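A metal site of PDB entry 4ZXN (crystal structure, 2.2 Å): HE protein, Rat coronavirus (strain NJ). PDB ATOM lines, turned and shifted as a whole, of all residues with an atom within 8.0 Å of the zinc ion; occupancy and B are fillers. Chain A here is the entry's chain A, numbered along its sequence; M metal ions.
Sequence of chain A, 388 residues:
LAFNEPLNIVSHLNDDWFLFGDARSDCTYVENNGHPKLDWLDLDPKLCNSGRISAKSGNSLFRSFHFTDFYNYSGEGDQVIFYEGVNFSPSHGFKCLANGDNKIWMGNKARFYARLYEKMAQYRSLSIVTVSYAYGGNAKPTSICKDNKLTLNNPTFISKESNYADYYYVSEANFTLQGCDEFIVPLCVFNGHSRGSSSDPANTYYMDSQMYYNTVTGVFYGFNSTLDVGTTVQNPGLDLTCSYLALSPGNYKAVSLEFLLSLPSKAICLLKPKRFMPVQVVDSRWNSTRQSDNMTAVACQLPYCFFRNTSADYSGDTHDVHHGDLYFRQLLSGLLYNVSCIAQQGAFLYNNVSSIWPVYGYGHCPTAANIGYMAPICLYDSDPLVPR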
ATOM      1  N   TYR A  29     -30.372  25.549  22.039  1.00  0.00           N
ATOM      2  CA  TYR A  29     -28.985  25.077  21.920  1.00  0.00           C
ATOM      3  C   TYR A  29     -28.286  25.050  23.279  1.00  0.00           C
ATOM      4  O   TYR A  29     -28.483  25.941  24.109  1.00  0.00           O
ATOM      5  CB  TYR A  29     -28.213  25.949  20.925  1.00  0.00           C
ATOM      6  CG  TYR A  29     -26.754  25.574  20.731  1.00  0.00           C
ATOM      7  CD1 TYR A  29     -26.390  24.499  19.923  1.00  0.00           C
ATOM      8  CD2 TYR A  29     -25.733  26.305  21.343  1.00  0.00           C
ATOM      9  CE1 TYR A  29     -25.054  24.153  19.741  1.00  0.00           C
ATOM     10  CE2 TYR A  29     -24.399  25.976  21.171  1.00  0.00           C
ATOM     11  CZ  TYR A  29     -24.064  24.893  20.372  1.00  0.00           C
ATOM     12  OH  TYR A  29     -22.740  24.563  20.199  1.00  0.00           O
ATOM     13  N   VAL A  30     -27.471  24.020  23.491  1.00  0.00           N
ATOM     14  CA  VAL A  30     -26.757  23.824  24.763  1.00  0.00           C
ATOM     15  C   VAL A  30     -25.240  23.815  24.570  1.00  0.00           C
ATOM     16  O   VAL A  30     -24.742  23.374  23.533  1.00  0.00           O
ATOM     17  CB  VAL A  30     -27.212  22.539  25.499  1.00  0.00           C
ATOM     18  CG1 VAL A  30     -28.620  22.700  26.064  1.00  0.00           C
ATOM     19  CG2 VAL A  30     -27.135  21.314  24.585  1.00  0.00           C
ATOM     20  N   GLU A  31     -24.527  24.298  25.576  1.00  0.00           N
ATOM     21  CA  GLU A  31     -23.058  24.261  25.601  1.00  0.00           C
ATOM     22  C   GLU A  31     -22.517  24.206  27.022  1.00  0.00           C
ATOM     23  O   GLU A  31     -23.025  24.875  27.926  1.00  0.00           O
ATOM     24  CB  GLU A  31     -22.443  25.446  24.821  1.00  0.00           C
ATOM     25  CG  GLU A  31     -22.906  26.824  25.278  1.00  0.00           C
ATOM     26  CD  GLU A  31     -22.238  27.972  24.531  1.00  0.00           C
ATOM     27  OE1 GLU A  31     -21.486  27.725  23.558  1.00  0.00           O
ATOM     28  OE2 GLU A  31     -22.471  29.132  24.917  1.00  0.00           O
ATOM     29  N   ASN A  32     -21.480  23.390  27.220  1.00  0.00           N
ATOM     30  CA  ASN A  32     -20.830  23.241  28.522  1.00  0.00           C
ATOM     31  C   ASN A  32     -19.430  23.870  28.511  1.00  0.00           C
ATOM     32  O   ASN A  32     -18.436  23.185  28.300  1.00  0.00           O
ATOM     33  CB  ASN A  32     -20.777  21.770  28.937  1.00  0.00           C
ATOM     34  CG  ASN A  32     -20.263  21.565  30.354  1.00  0.00           C
ATOM     35  OD1 ASN A  32     -20.542  22.363  31.250  1.00  0.00           O
ATOM     36  ND2 ASN A  32     -19.523  20.483  30.564  1.00  0.00           N
ATOM     37  N   ASN A  33     -19.386  25.187  28.730  1.00  0.00           N
ATOM     38  CA  ASN A  33     -18.129  25.952  28.724  1.00  0.00           C
ATOM     39  C   ASN A  33     -18.235  27.279  29.479  1.00  0.00           C
ATOM     40  O   ASN A  33     -19.263  27.569  30.098  1.00  0.00           O
ATOM     41  CB  ASN A  33     -17.621  26.172  27.295  1.00  0.00           C
ATOM     42  CG  ASN A  33     -18.734  26.573  26.327  1.00  0.00           C
ATOM     43  OD1 ASN A  33     -19.800  27.051  26.721  1.00  0.00           O
ATOM     44  ND2 ASN A  33     -18.471  26.389  25.035  1.00  0.00           N
ATOM     45  N   GLY A  34     -17.172  28.079  29.423  1.00  0.00           N
ATOM     46  CA  GLY A  34     -17.126  29.385  30.076  1.00  0.00           C
ATOM     47  C   GLY A  34     -17.652  30.525  29.205  1.00  0.00           C
ATOM     48  O   GLY A  34     -17.191  31.661  29.319  1.00  0.00           O
ATOM     49  N   HIS A  35     -18.610  30.196  28.336  1.00  0.00           N
ATOM     50  CA  HIS A  35     -19.232  31.175  27.446  1.00  0.00           C
ATOM     51  C   HIS A  35     -20.324  31.962  28.161  1.00  0.00           C
ATOM     52  O   HIS A  35     -20.948  31.454  29.093  1.00  0.00           O
ATOM     53  CB  HIS A  35     -19.854  30.452  26.248  1.00  0.00           C
ATOM     54  CG  HIS A  35     -18.882  30.106  25.159  1.00  0.00           C
ATOM     55  ND1 HIS A  35     -19.214  30.178  23.818  1.00  0.00           N
ATOM     56  CD2 HIS A  35     -17.591  29.705  25.203  1.00  0.00           C
ATOM     57  CE1 HIS A  35     -18.171  29.823  23.091  1.00  0.00           C
ATOM     58  NE2 HIS A  35     -17.169  29.535  23.911  1.00  0.00           N
ATOM     59  N   PRO A  36     -20.567  33.211  27.720  1.00  0.00           N
ATOM     60  CA  PRO A  36     -21.737  33.959  28.173  1.00  0.00           C
ATOM     61  C   PRO A  36     -23.033  33.284  27.724  1.00  0.00           C
ATOM     62  O   PRO A  36     -23.060  32.650  26.661  1.00  0.00           O
ATOM     63  CB  PRO A  36     -21.589  35.315  27.471  1.00  0.00           C
ATOM     64  CG  PRO A  36     -20.125  35.440  27.198  1.00  0.00           C
ATOM     65  CD  PRO A  36     -19.680  34.047  26.884  1.00  0.00           C
ATOM     66  N   LYS A  37     -24.086  33.411  28.539  1.00  0.00           N
ATOM     67  CA  LYS A  37     -25.366  32.777  28.241  1.00  0.00           C
ATOM     68  C   LYS A  37     -25.912  33.222  26.885  1.00  0.00           C
ATOM     69  O   LYS A  37     -25.939  34.415  26.573  1.00  0.00           O
ATOM     70  CB  LYS A  37     -26.384  33.086  29.345  1.00  0.00           C
ATOM     71  CG  LYS A  37     -26.119  32.414  30.689  1.00  0.00           C
ATOM     72  CD  LYS A  37     -26.408  30.924  30.648  1.00  0.00           C
ATOM     73  CE  LYS A  37     -26.236  30.278  32.012  1.00  0.00           C
ATOM     74  NZ  LYS A  37     -27.365  30.589  32.939  1.00  0.00           N
ATOM     75  N   LEU A  38     -26.308  32.232  26.076  1.00  0.00           N
ATOM     76  CA  LEU A  38     -26.955  32.463  24.774  1.00  0.00           C
ATOM     77  C   LEU A  38     -26.130  33.316  23.801  1.00  0.00           C
ATOM     78  O   LEU A  38     -26.692  34.074  22.999  1.00  0.00           O
ATOM     79  CB  LEU A  38     -28.372  33.045  24.959  1.00  0.00           C
ATOM     80  CG  LEU A  38     -29.395  32.272  25.806  1.00  0.00           C
ATOM     81  CD1 LEU A  38     -30.529  33.192  26.229  1.00  0.00           C
ATOM     82  CD2 LEU A  38     -29.930  31.049  25.076  1.00  0.00           C
ATOM     83  N   ASP A  39     -24.813  33.177  23.856  1.00  0.00           N
ATOM     84  CA  ASP A  39     -23.909  34.050  23.098  1.00  0.00           C
ATOM     85  C   ASP A  39     -23.837  33.755  21.591  1.00  0.00           C
ATOM     86  O   ASP A  39     -23.267  34.536  20.820  1.00  0.00           O
ATOM     87  CB  ASP A  39     -22.504  34.076  23.719  1.00  0.00           C
ATOM     88  CG  ASP A  39     -21.744  32.756  23.546  1.00  0.00           C
ATOM     89  OD1 ASP A  39     -22.373  31.700  23.349  1.00  0.00           O
ATOM     90  OD2 ASP A  39     -20.503  32.798  23.619  1.00  0.00           O
ATOM     91  N   TRP A  40     -24.420  32.627  21.186  1.00  0.00           N
ATOM     92  CA  TRP A  40     -24.471  32.243  19.772  1.00  0.00           C
ATOM     93  C   TRP A  40     -25.601  32.957  19.022  1.00  0.00           C
ATOM     94  O   TRP A  40     -25.653  32.930  17.793  1.00  0.00           O
ATOM     95  CB  TRP A  40     -24.637  30.729  19.653  1.00  0.00           C
ATOM     96  CG  TRP A  40     -25.862  30.192  20.346  1.00  0.00           C
ATOM     97  CD1 TRP A  40     -27.093  30.011  19.799  1.00  0.00           C
ATOM     98  CD2 TRP A  40     -25.963  29.787  21.715  1.00  0.00           C
ATOM     99  NE1 TRP A  40     -27.959  29.512  20.737  1.00  0.00           N
ATOM    100  CE2 TRP A  40     -27.299  29.362  21.923  1.00  0.00           C
ATOM    101  CE3 TRP A  40     -25.062  29.747  22.789  1.00  0.00           C
ATOM    102  CZ2 TRP A  40     -27.756  28.898  23.161  1.00  0.00           C
ATOM    103  CZ3 TRP A  40     -25.518  29.275  24.021  1.00  0.00           C
ATOM    104  CH2 TRP A  40     -26.856  28.856  24.199  1.00  0.00           C
ATOM    105  N   LEU A  41     -26.499  33.597  19.780  1.00  0.00           N
ATOM    106  CA  LEU A  41     -27.692  34.234  19.209  1.00  0.00           C
ATOM    107  C   LEU A  41     -27.414  35.592  18.582  1.00  0.00           C
ATOM    108  O   LEU A  41     -26.588  36.367  19.069  1.00  0.00           O
ATOM    109  CB  LEU A  41     -28.776  34.382  20.281  1.00  0.00           C
ATOM    110  CG  LEU A  41     -29.519  33.155  20.835  1.00  0.00           C
ATOM    111  CD1 LEU A  41     -30.488  33.596  21.921  1.00  0.00           C
ATOM    112  CD2 LEU A  41     -30.247  32.392  19.748  1.00  0.00           C
ATOM    113  N   THR A 318     -18.324  36.307  20.838  1.00  0.00           N
ATOM    114  CA  THR A 318     -17.700  35.416  21.814  1.00  0.00           C
ATOM    115  C   THR A 318     -17.838  33.921  21.508  1.00  0.00           C
ATOM    116  O   THR A 318     -16.944  33.137  21.848  1.00  0.00           O
ATOM    117  CB  THR A 318     -18.210  35.668  23.251  1.00  0.00           C
ATOM    118  OG1 THR A 318     -19.641  35.729  23.250  1.00  0.00           O
ATOM    119  CG2 THR A 318     -17.642  36.973  23.806  1.00  0.00           C
ATOM    120  N   HIS A 319     -18.940  33.526  20.887  1.00  0.00           N
ATOM    121  CA  HIS A 319     -19.186  32.117  20.578  1.00  0.00           C
ATOM    122  C   HIS A 319     -18.168  31.586  19.553  1.00  0.00           C
ATOM    123  O   HIS A 319     -17.338  30.734  19.880  1.00  0.00           O
ATOM    124  CB  HIS A 319     -20.624  31.895  20.088  1.00  0.00           C
ATOM    125  CG  HIS A 319     -20.977  30.453  19.917  1.00  0.00           C
ATOM    126  ND1 HIS A 319     -21.210  29.602  20.975  1.00  0.00           N
ATOM    127  CD2 HIS A 319     -21.115  29.704  18.794  1.00  0.00           C
ATOM    128  CE1 HIS A 319     -21.485  28.401  20.523  1.00  0.00           C
ATOM    129  NE2 HIS A 319     -21.441  28.425  19.202  1.00  0.00           N
ATOM    130  N   ASP A 320     -18.276  32.076  18.326  1.00  0.00           N
ATOM    131  CA  ASP A 320     -17.257  31.879  17.287  1.00  0.00           C
ATOM    132  C   ASP A 320     -17.390  32.997  16.254  1.00  0.00           C
ATOM    133  O   ASP A 320     -18.204  33.908  16.423  1.00  0.00           O
ATOM    134  CB  ASP A 320     -17.346  30.483  16.642  1.00  0.00           C
ATOM    135  CG  ASP A 320     -18.707  30.196  16.016  1.00  0.00           C
ATOM    136  OD1 ASP A 320     -19.353  31.114  15.486  1.00  0.00           O
ATOM    137  OD2 ASP A 320     -19.135  29.022  16.052  1.00  0.00           O
ATOM    138  N   HIS A 323     -21.158  33.311  14.721  1.00  0.00           N
ATOM    139  CA  HIS A 323     -22.346  33.492  15.564  1.00  0.00           C
ATOM    140  C   HIS A 323     -22.229  34.691  16.510  1.00  0.00           C
ATOM    141  O   HIS A 323     -21.244  34.812  17.244  1.00  0.00           O
ATOM    142  CB  HIS A 323     -22.633  32.229  16.385  1.00  0.00           C
ATOM    143  CG  HIS A 323     -22.877  31.003  15.546  1.00  0.00           C
ATOM    144  ND1 HIS A 323     -21.860  30.171  15.133  1.00  0.00           N
ATOM    145  CD2 HIS A 323     -24.027  30.488  15.043  1.00  0.00           C
ATOM    146  CE1 HIS A 323     -22.367  29.188  14.415  1.00  0.00           C
ATOM    147  NE2 HIS A 323     -23.677  29.346  14.347  1.00  0.00           N
HETATM  148 ZN    ZN M   1     -21.140  30.017  22.834  1.00  0.00          ZN
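Merely in contact with the zinc ion: Trp 40. Five residues have an atom within 4 Å of the zinc ion: Glu 31, His 35, Asp 39, Trp 40 and His 319. The nearest printed residue that does not touch the zinc ion is Asn 33 (5.0 Å).
The side-chain hydroxyl (OG1) of Thr 318 is in hydrogen-bond range of the side-chain carboxylate (OD2) of Asp 39, at 3.1 Å.
The zinc ion is bound by ND1 of His 319 (1.9 Å), OD1 of Asp 39 (2.1 Å), ND1 of His 35 (2.2 Å) and OE1 of Glu 31 (2.4 Å). Slightly farther from the zinc ion lies the side-chain carboxylate (OE2) of Glu 31 (2.6 Å).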
